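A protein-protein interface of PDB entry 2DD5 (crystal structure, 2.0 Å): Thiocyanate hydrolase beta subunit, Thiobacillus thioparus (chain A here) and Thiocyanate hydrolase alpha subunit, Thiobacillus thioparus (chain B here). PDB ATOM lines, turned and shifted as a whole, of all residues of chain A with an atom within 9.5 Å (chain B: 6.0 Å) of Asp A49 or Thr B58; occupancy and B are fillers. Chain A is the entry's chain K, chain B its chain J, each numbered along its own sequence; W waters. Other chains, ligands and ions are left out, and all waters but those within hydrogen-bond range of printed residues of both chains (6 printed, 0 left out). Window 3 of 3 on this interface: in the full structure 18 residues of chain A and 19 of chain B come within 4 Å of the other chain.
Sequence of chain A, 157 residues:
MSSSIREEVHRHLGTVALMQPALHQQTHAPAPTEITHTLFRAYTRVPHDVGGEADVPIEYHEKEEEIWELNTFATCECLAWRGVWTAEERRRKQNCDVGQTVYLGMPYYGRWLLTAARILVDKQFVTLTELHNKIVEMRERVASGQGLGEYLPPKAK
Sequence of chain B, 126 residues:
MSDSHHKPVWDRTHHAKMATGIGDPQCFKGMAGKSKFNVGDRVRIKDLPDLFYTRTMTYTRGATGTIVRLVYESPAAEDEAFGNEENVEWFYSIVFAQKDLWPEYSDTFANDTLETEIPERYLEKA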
ATOM      1  N   ARG A  41      -3.470  14.951  -0.746  1.00  0.00           N
ATOM      2  CA  ARG A  41      -3.122  14.255  -1.979  1.00  0.00           C
ATOM      3  C   ARG A  41      -2.251  13.035  -1.700  1.00  0.00           C
ATOM      4  O   ARG A  41      -2.394  12.003  -2.356  1.00  0.00           O
ATOM      5  CB  ARG A  41      -2.398  15.198  -2.954  1.00  0.00           C
ATOM      6  CG  ARG A  41      -1.910  14.494  -4.225  1.00  0.00           C
ATOM      7  CD  ARG A  41      -1.636  15.462  -5.377  1.00  0.00           C
ATOM      8  NE  ARG A  41      -1.263  14.744  -6.598  1.00  0.00           N
ATOM      9  CZ  ARG A  41      -1.325  15.259  -7.825  1.00  0.00           C
ATOM     10  NH1 ARG A  41      -1.747  16.505  -8.008  1.00  0.00           N
ATOM     11  NH2 ARG A  41      -0.970  14.522  -8.874  1.00  0.00           N
ATOM     12  N   ALA A  42      -1.354  13.153  -0.728  1.00  0.00           N
ATOM     13  CA  ALA A  42      -0.473  12.049  -0.379  1.00  0.00           C
ATOM     14  C   ALA A  42      -1.257  10.894   0.252  1.00  0.00           C
ATOM     15  O   ALA A  42      -1.018   9.729  -0.063  1.00  0.00           O
ATOM     16  CB  ALA A  42       0.625  12.529   0.575  1.00  0.00           C
ATOM     17  N   THR A  44      -4.545  10.238  -0.086  1.00  0.00           N
ATOM     18  CA  THR A  44      -5.534   9.677  -1.003  1.00  0.00           C
ATOM     19  C   THR A  44      -4.902   9.158  -2.289  1.00  0.00           C
ATOM     20  O   THR A  44      -5.591   8.902  -3.277  1.00  0.00           O
ATOM     21  CB  THR A  44      -6.624  10.712  -1.355  1.00  0.00           C
ATOM     22  OG1 THR A  44      -6.023  11.864  -1.958  1.00  0.00           O
ATOM     23  CG2 THR A  44      -7.376  11.141  -0.093  1.00  0.00           C
ATOM     24  N   ARG A  45      -3.583   8.999  -2.263  1.00  0.00           N
ATOM     25  CA  ARG A  45      -2.837   8.492  -3.413  1.00  0.00           C
ATOM     26  C   ARG A  45      -3.245   7.050  -3.687  1.00  0.00           C
ATOM     27  O   ARG A  45      -3.848   6.390  -2.841  1.00  0.00           O
ATOM     28  CB  ARG A  45      -1.338   8.485  -3.106  1.00  0.00           C
ATOM     29  CG  ARG A  45      -0.990   7.429  -2.048  1.00  0.00           C
ATOM     30  CD  ARG A  45       0.502   7.219  -1.836  1.00  0.00           C
ATOM     31  NE  ARG A  45       1.169   6.703  -3.027  1.00  0.00           N
ATOM     32  CZ  ARG A  45       2.385   6.168  -3.028  1.00  0.00           C
ATOM     33  NH1 ARG A  45       3.072   6.068  -1.897  1.00  0.00           N
ATOM     34  NH2 ARG A  45       2.926   5.752  -4.163  1.00  0.00           N
ATOM     35  N   VAL A  46      -2.898   6.568  -4.874  1.00  0.00           N
ATOM     36  CA  VAL A  46      -3.153   5.188  -5.254  1.00  0.00           C
ATOM     37  C   VAL A  46      -1.792   4.543  -4.951  1.00  0.00           C
ATOM     38  O   VAL A  46      -0.793   4.862  -5.593  1.00  0.00           O
ATOM     39  CB  VAL A  46      -3.488   5.087  -6.760  1.00  0.00           C
ATOM     40  CG1 VAL A  46      -3.861   3.679  -7.113  1.00  0.00           C
ATOM     41  CG2 VAL A  46      -4.647   6.014  -7.095  1.00  0.00           C
ATOM     42  N   PRO A  47      -1.737   3.643  -3.954  1.00  0.00           N
ATOM     43  CA  PRO A  47      -0.521   2.943  -3.517  1.00  0.00           C
ATOM     44  C   PRO A  47       0.428   2.356  -4.560  1.00  0.00           C
ATOM     45  O   PRO A  47       1.647   2.400  -4.377  1.00  0.00           O
ATOM     46  CB  PRO A  47      -1.067   1.861  -2.585  1.00  0.00           C
ATOM     47  CG  PRO A  47      -2.272   2.514  -1.996  1.00  0.00           C
ATOM     48  CD  PRO A  47      -2.909   3.143  -3.213  1.00  0.00           C
ATOM     49  N   HIS A  48      -0.116   1.815  -5.647  1.00  0.00           N
ATOM     50  CA  HIS A  48       0.725   1.180  -6.655  1.00  0.00           C
ATOM     51  C   HIS A  48       1.546   2.114  -7.539  1.00  0.00           C
ATOM     52  O   HIS A  48       2.469   1.667  -8.216  1.00  0.00           O
ATOM     53  CB  HIS A  48      -0.118   0.239  -7.534  1.00  0.00           C
ATOM     54  CG  HIS A  48      -1.064   0.934  -8.470  1.00  0.00           C
ATOM     55  ND1 HIS A  48      -1.813   0.249  -9.403  1.00  0.00           N
ATOM     56  CD2 HIS A  48      -1.375   2.243  -8.630  1.00  0.00           C
ATOM     57  CE1 HIS A  48      -2.542   1.104 -10.099  1.00  0.00           C
ATOM     58  NE2 HIS A  48      -2.294   2.322  -9.649  1.00  0.00           N
ATOM     59  N   ASP A  49       1.230   3.406  -7.513  1.00  0.00           N
ATOM     60  CA  ASP A  49       1.929   4.384  -8.350  1.00  0.00           C
ATOM     61  C   ASP A  49       3.234   4.849  -7.699  1.00  0.00           C
ATOM     62  O   ASP A  49       3.290   5.928  -7.109  1.00  0.00           O
ATOM     63  CB  ASP A  49       1.000   5.572  -8.590  1.00  0.00           C
ATOM     64  CG  ASP A  49       1.518   6.518  -9.648  1.00  0.00           C
ATOM     65  OD1 ASP A  49       2.529   6.199 -10.307  1.00  0.00           O
ATOM     66  OD2 ASP A  49       0.894   7.582  -9.825  1.00  0.00           O
ATOM     67  N   VAL A  50       4.285   4.046  -7.832  1.00  0.00           N
ATOM     68  CA  VAL A  50       5.567   4.362  -7.203  1.00  0.00           C
ATOM     69  C   VAL A  50       6.694   4.867  -8.116  1.00  0.00           C
ATOM     70  O   VAL A  50       7.754   5.256  -7.629  1.00  0.00           O
ATOM     71  CB  VAL A  50       6.086   3.131  -6.425  1.00  0.00           C
ATOM     72  CG1 VAL A  50       4.990   2.619  -5.459  1.00  0.00           C
ATOM     73  CG2 VAL A  50       6.491   2.025  -7.401  1.00  0.00           C
ATOM     74  N   GLY A  51       6.466   4.869  -9.427  1.00  0.00           N
ATOM     75  CA  GLY A  51       7.497   5.312 -10.357  1.00  0.00           C
ATOM     76  C   GLY A  51       8.076   6.689 -10.065  1.00  0.00           C
ATOM     77  O   GLY A  51       7.339   7.662  -9.941  1.00  0.00           O
ATOM     78  N   GLY A  52       9.398   6.773  -9.950  1.00  0.00           N
ATOM     79  CA  GLY A  52      10.027   8.056  -9.685  1.00  0.00           C
ATOM     80  C   GLY A  52      10.371   8.321  -8.230  1.00  0.00           C
ATOM     81  O   GLY A  52      11.088   9.278  -7.932  1.00  0.00           O
ATOM     82  N   GLU A  53       9.870   7.492  -7.317  1.00  0.00           N
ATOM     83  CA  GLU A  53      10.169   7.682  -5.900  1.00  0.00           C
ATOM     84  C   GLU A  53      11.623   7.314  -5.647  1.00  0.00           C
ATOM     85  O   GLU A  53      12.134   6.350  -6.206  1.00  0.00           O
ATOM     86  CB  GLU A  53       9.260   6.807  -5.030  1.00  0.00           C
ATOM     87  CG  GLU A  53       7.791   7.204  -5.055  1.00  0.00           C
ATOM     88  CD  GLU A  53       6.908   6.226  -4.288  1.00  0.00           C
ATOM     89  OE1 GLU A  53       7.450   5.323  -3.618  1.00  0.00           O
ATOM     90  OE2 GLU A  53       5.669   6.368  -4.353  1.00  0.00           O
ATOM     91  N   ARG A  91      -6.373  -5.996 -10.011  1.00  0.00           N
ATOM     92  CA  ARG A  91      -5.301  -5.036  -9.747  1.00  0.00           C
ATOM     93  C   ARG A  91      -5.745  -3.916  -8.815  1.00  0.00           C
ATOM     94  O   ARG A  91      -5.039  -3.573  -7.868  1.00  0.00           O
ATOM     95  CB  ARG A  91      -4.771  -4.441 -11.057  1.00  0.00           C
ATOM     96  CG  ARG A  91      -4.034  -5.450 -11.926  1.00  0.00           C
ATOM     97  CD  ARG A  91      -3.295  -4.796 -13.099  1.00  0.00           C
ATOM     98  NE  ARG A  91      -2.722  -5.832 -13.954  1.00  0.00           N
ATOM     99  CZ  ARG A  91      -3.364  -6.401 -14.969  1.00  0.00           C
ATOM    100  NH1 ARG A  91      -4.594  -6.016 -15.278  1.00  0.00           N
ATOM    101  NH2 ARG A  91      -2.802  -7.405 -15.634  1.00  0.00           N
ATOM    102  N   ASN A  95      -3.616  -4.127  -5.602  1.00  0.00           N
ATOM    103  CA  ASN A  95      -2.493  -3.208  -5.529  1.00  0.00           C
ATOM    104  C   ASN A  95      -2.830  -1.811  -5.031  1.00  0.00           C
ATOM    105  O   ASN A  95      -1.933  -0.985  -4.848  1.00  0.00           O
ATOM    106  CB  ASN A  95      -1.833  -3.107  -6.907  1.00  0.00           C
ATOM    107  CG  ASN A  95      -1.526  -4.465  -7.506  1.00  0.00           C
ATOM    108  OD1 ASN A  95      -1.068  -5.366  -6.812  1.00  0.00           O
ATOM    109  ND2 ASN A  95      -1.772  -4.614  -8.807  1.00  0.00           N
ATOM    110  N   CYS A  96      -4.113  -1.544  -4.819  1.00  0.00           N
ATOM    111  CA  CYS A  96      -4.533  -0.223  -4.369  1.00  0.00           C
ATOM    112  C   CYS A  96      -5.430  -0.251  -3.136  1.00  0.00           C
ATOM    113  O   CYS A  96      -5.104   0.366  -2.127  1.00  0.00           O
ATOM    114  CB  CYS A  96      -5.239   0.510  -5.517  1.00  0.00           C
ATOM    115  SG  CYS A  96      -4.192   0.680  -6.997  1.00  0.00           S
ATOM    116  N   GLN A 100      -1.728   1.532   1.895  1.00  0.00           N
ATOM    117  CA  GLN A 100      -0.280   1.697   1.996  1.00  0.00           C
ATOM    118  C   GLN A 100       0.462   0.708   2.895  1.00  0.00           C
ATOM    119  O   GLN A 100       1.474   0.134   2.491  1.00  0.00           O
ATOM    120  CB  GLN A 100       0.032   3.119   2.465  1.00  0.00           C
ATOM    121  CG  GLN A 100       1.507   3.469   2.485  1.00  0.00           C
ATOM    122  CD  GLN A 100       2.094   3.579   1.090  1.00  0.00           C
ATOM    123  OE1 GLN A 100       2.252   2.582   0.385  1.00  0.00           O
ATOM    124  NE2 GLN A 100       2.405   4.798   0.681  1.00  0.00           N
ATOM    125  N   TYR A 103       0.233  -2.834   1.542  1.00  0.00           N
ATOM    126  CA  TYR A 103       0.852  -2.807   0.224  1.00  0.00           C
ATOM    127  C   TYR A 103       2.361  -3.049   0.263  1.00  0.00           C
ATOM    128  O   TYR A 103       2.897  -3.793  -0.560  1.00  0.00           O
ATOM    129  CB  TYR A 103       0.568  -1.472  -0.473  1.00  0.00           C
ATOM    130  CG  TYR A 103       1.052  -1.455  -1.907  1.00  0.00           C
ATOM    131  CD1 TYR A 103       0.527  -2.349  -2.845  1.00  0.00           C
ATOM    132  CD2 TYR A 103       2.072  -0.593  -2.313  1.00  0.00           C
ATOM    133  CE1 TYR A 103       1.007  -2.390  -4.151  1.00  0.00           C
ATOM    134  CE2 TYR A 103       2.567  -0.627  -3.628  1.00  0.00           C
ATOM    135  CZ  TYR A 103       2.030  -1.529  -4.535  1.00  0.00           C
ATOM    136  OH  TYR A 103       2.520  -1.599  -5.821  1.00  0.00           O
ATOM    137  N   LEU A 104       3.050  -2.437   1.219  1.00  0.00           N
ATOM    138  CA  LEU A 104       4.497  -2.609   1.313  1.00  0.00           C
ATOM    139  C   LEU A 104       4.944  -3.512   2.461  1.00  0.00           C
ATOM    140  O   LEU A 104       6.092  -3.963   2.494  1.00  0.00           O
ATOM    141  CB  LEU A 104       5.171  -1.235   1.415  1.00  0.00           C
ATOM    142  CG  LEU A 104       5.088  -0.411   0.122  1.00  0.00           C
ATOM    143  CD1 LEU A 104       5.583   1.012   0.359  1.00  0.00           C
ATOM    144  CD2 LEU A 104       5.933  -1.092  -0.953  1.00  0.00           C
ATOM    145  N   ASP B  50      -7.293  11.283  -9.336  1.00  0.00           N
ATOM    146  CA  ASP B  50      -7.092   9.843  -9.399  1.00  0.00           C
ATOM    147  C   ASP B  50      -7.586   9.115  -8.156  1.00  0.00           C
ATOM    148  O   ASP B  50      -7.135   8.016  -7.843  1.00  0.00           O
ATOM    149  CB  ASP B  50      -5.621   9.506  -9.658  1.00  0.00           C
ATOM    150  CG  ASP B  50      -4.681  10.241  -8.742  1.00  0.00           C
ATOM    151  OD1 ASP B  50      -4.988  10.357  -7.535  1.00  0.00           O
ATOM    152  OD2 ASP B  50      -3.622  10.691  -9.229  1.00  0.00           O
ATOM    153  N   THR B  54      -6.298   4.736 -10.858  1.00  0.00           N
ATOM    154  CA  THR B  54      -5.831   5.312 -12.114  1.00  0.00           C
ATOM    155  C   THR B  54      -4.629   4.502 -12.568  1.00  0.00           C
ATOM    156  O   THR B  54      -3.922   3.917 -11.744  1.00  0.00           O
ATOM    157  CB  THR B  54      -5.370   6.785 -11.976  1.00  0.00           C
ATOM    158  OG1 THR B  54      -4.981   7.281 -13.268  1.00  0.00           O
ATOM    159  CG2 THR B  54      -4.169   6.890 -11.038  1.00  0.00           C
ATOM    160  N   THR B  56      -2.586   6.004 -14.962  1.00  0.00           N
ATOM    161  CA  THR B  56      -1.771   7.030 -15.617  1.00  0.00           C
ATOM    162  C   THR B  56      -0.886   7.556 -14.499  1.00  0.00           C
ATOM    163  O   THR B  56      -1.312   8.364 -13.676  1.00  0.00           O
ATOM    164  CB  THR B  56      -2.630   8.169 -16.202  1.00  0.00           C
ATOM    165  OG1 THR B  56      -3.510   7.631 -17.194  1.00  0.00           O
ATOM    166  CG2 THR B  56      -1.743   9.229 -16.858  1.00  0.00           C
ATOM    167  N   MET B  57       0.348   7.065 -14.468  1.00  0.00           N
ATOM    168  CA  MET B  57       1.303   7.416 -13.434  1.00  0.00           C
ATOM    169  C   MET B  57       1.431   8.899 -13.139  1.00  0.00           C
ATOM    170  O   MET B  57       1.400   9.743 -14.036  1.00  0.00           O
ATOM    171  CB  MET B  57       2.690   6.860 -13.778  1.00  0.00           C
ATOM    172  CG  MET B  57       2.752   5.347 -13.959  1.00  0.00           C
ATOM    173  SD  MET B  57       1.933   4.741 -15.454  1.00  0.00           S
ATOM    174  CE  MET B  57       3.091   5.268 -16.739  1.00  0.00           C
ATOM    175  N   THR B  58       1.579   9.196 -11.855  1.00  0.00           N
ATOM    176  CA  THR B  58       1.751  10.558 -11.384  1.00  0.00           C
ATOM    177  C   THR B  58       2.949  11.214 -12.077  1.00  0.00           C
ATOM    178  O   THR B  58       2.907  12.399 -12.405  1.00  0.00           O
ATOM    179  CB  THR B  58       1.991  10.575  -9.849  1.00  0.00           C
ATOM    180  OG1 THR B  58       0.808  10.123  -9.177  1.00  0.00           O
ATOM    181  CG2 THR B  58       2.343  11.979  -9.368  1.00  0.00           C
ATOM    182  N   TYR B  59       4.011  10.449 -12.320  1.00  0.00           N
ATOM    183  CA  TYR B  59       5.195  11.037 -12.942  1.00  0.00           C
ATOM    184  C   TYR B  59       4.982  11.598 -14.349  1.00  0.00           C
ATOM    185  O   TYR B  59       5.803  12.376 -14.836  1.00  0.00           O
ATOM    186  CB  TYR B  59       6.381  10.050 -12.904  1.00  0.00           C
ATOM    187  CG  TYR B  59       6.333   8.863 -13.852  1.00  0.00           C
ATOM    188  CD1 TYR B  59       6.564   9.026 -15.218  1.00  0.00           C
ATOM    189  CD2 TYR B  59       6.119   7.566 -13.370  1.00  0.00           C
ATOM    190  CE1 TYR B  59       6.589   7.924 -16.089  1.00  0.00           C
ATOM    191  CE2 TYR B  59       6.139   6.456 -14.233  1.00  0.00           C
ATOM    192  CZ  TYR B  59       6.377   6.648 -15.589  1.00  0.00           C
ATOM    193  OH  TYR B  59       6.414   5.565 -16.443  1.00  0.00           O
ATOM    194  N   THR B  60       3.875  11.242 -14.998  1.00  0.00           N
ATOM    195  CA  THR B  60       3.611  11.757 -16.344  1.00  0.00           C
ATOM    196  C   THR B  60       2.722  13.006 -16.376  1.00  0.00           C
ATOM    197  O   THR B  60       2.646  13.684 -17.399  1.00  0.00           O
ATOM    198  CB  THR B  60       2.902  10.720 -17.231  1.00  0.00           C
ATOM    199  OG1 THR B  60       1.569  10.530 -16.746  1.00  0.00           O
ATOM    200  CG2 THR B  60       3.646   9.393 -17.223  1.00  0.00           C
ATOM    201  N   ARG B  61       2.053  13.315 -15.269  1.00  0.00           N
ATOM    202  CA  ARG B  61       1.140  14.455 -15.238  1.00  0.00           C
ATOM    203  C   ARG B  61       1.786  15.796 -15.583  1.00  0.00           C
ATOM    204  O   ARG B  61       2.821  16.158 -15.031  1.00  0.00           O
ATOM    205  CB  ARG B  61       0.452  14.556 -13.867  1.00  0.00           C
ATOM    206  CG  ARG B  61      -0.217  13.261 -13.375  1.00  0.00           C
ATOM    207  CD  ARG B  61      -1.089  12.617 -14.450  1.00  0.00           C
ATOM    208  NE  ARG B  61      -1.740  11.382 -14.002  1.00  0.00           N
ATOM    209  CZ  ARG B  61      -2.904  11.328 -13.355  1.00  0.00           C
ATOM    210  NH1 ARG B  61      -3.565  12.443 -13.068  1.00  0.00           N
ATOM    211  NH2 ARG B  61      -3.419  10.152 -13.007  1.00  0.00           N
HETATM  212  O   HOH W   1      -1.656   7.887  -9.034  1.00  0.00           O
HETATM  213  O   HOH W   2      -6.495  10.910  -5.175  1.00  0.00           O
HETATM  214  O   HOH W   3      -3.822  11.873  -4.649  1.00  0.00           O
HETATM  215  O   HOH W   4      -0.342  12.130  -7.315  1.00  0.00           O
HETATM  216  O   HOH W   5       4.464   8.175 -10.413  1.00  0.00           O
HETATM  217  O   HOH W   6      -3.834  13.450  -9.999  1.00  0.00           O
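O of Thr B54 is in hydrogen-bond range of NE2 of His A48, at 3.1 Å. The side-chain hydroxyl (OG1) of Thr B58 lies within hydrogen-bond range of the side-chain carboxylate (OD2) of Asp A49 (2.6 Å).
Among the printed residues, merely in contact across the chains: Val A46 with Asp B50 (3.3 Å), Asp A49 with Met B57 (3.5 Å) and Gly A51 with Tyr B59 (3.6 Å).
Printed residues of chain A that touch a printed residue of chain B: Val A46, His A48, Asp A49 and Gly A51. Hydrophobic or aromatic side chains of chain A within 4 Å of the printed part of chain B: Val A46 and His A48. Printed residues of chain B that touch a printed residue of chain A: Asp B50, Thr B54, Met B57, Thr B58 and Tyr B59. Hydrophobic or aromatic side chains of chain B that line the printed part of chain A: Met B57 and Tyr B59. Among the printed residues, 5 pairs touch across the chains. Among the printed residues, no Asp or Glu carboxylate lies within 4 Å of a Lys or Arg side-chain nitrogen of the other chain.
NH2 of Arg A45 is in hydrogen-bond range of O of Asp A49 (3.0 Å). OD2 of Asp B50 is in salt-bridge range of NH2 of Arg B61, at 3.8 Å. O of Met B57 lies within hydrogen-bond range of OG1 of Thr B60 (2.8 Å). OG1 of Thr B54 sits at hydrogen-bond distance from N of Thr B56 (3.2 Å). The backbone NH (N) of His A48 is in hydrogen-bond range of the backbone carbonyl oxygen (O) of Asn A95 (3.4 Å). OG1 of Thr B54 is in hydrogen-bond range of NH2 of Arg B61 (3.3 Å).
Of the printed residues of chain A, Met B57 touches Asp A49. Printed residues of chain B within 4 Å of His A48: Thr B54 (3.1 Å). Printed residues of chain B within 4 Å of Gly A51: Tyr B59. Of the printed residues of chain A, Tyr B59 touches Gly A51 (3.6 Å). Of the printed residues of chain B, Val A46 touches Asp B50. Pro A47 touches none of the printed residues of chain B. Tyr A103 touches none of the printed residues of chain B.
Water W1 lies within hydrogen-bond range of OD2 of Asp A49, OG1 of Thr B58 and OD2 of Asp B50. Water W3 lies within hydrogen-bond range of O of Arg A41, OD1 of Asp B50 and OG1 of Thr A44. Water W5 lies within hydrogen-bond range of the side-chain carboxylate of Asp A49, the backbone carbonyl oxygen of Gly A51, the backbone NH of Tyr B59 and the backbone NH of Thr B58. Water W2 lies within hydrogen-bond range of the side-chain carboxylate (OD1) of Asp B50 and the backbone carbonyl oxygen (O) of Thr A44. Water W4 lies within hydrogen-bond range of the guanidinium group (NE) of Arg A41 (2.9 Å) and the side-chain hydroxyl (OG1) of Thr B58 (3.0 Å). Water W6 lies within hydrogen-bond range of OD2 of Asp B50, NH1 of Arg B61 and NH2 of Arg A41.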
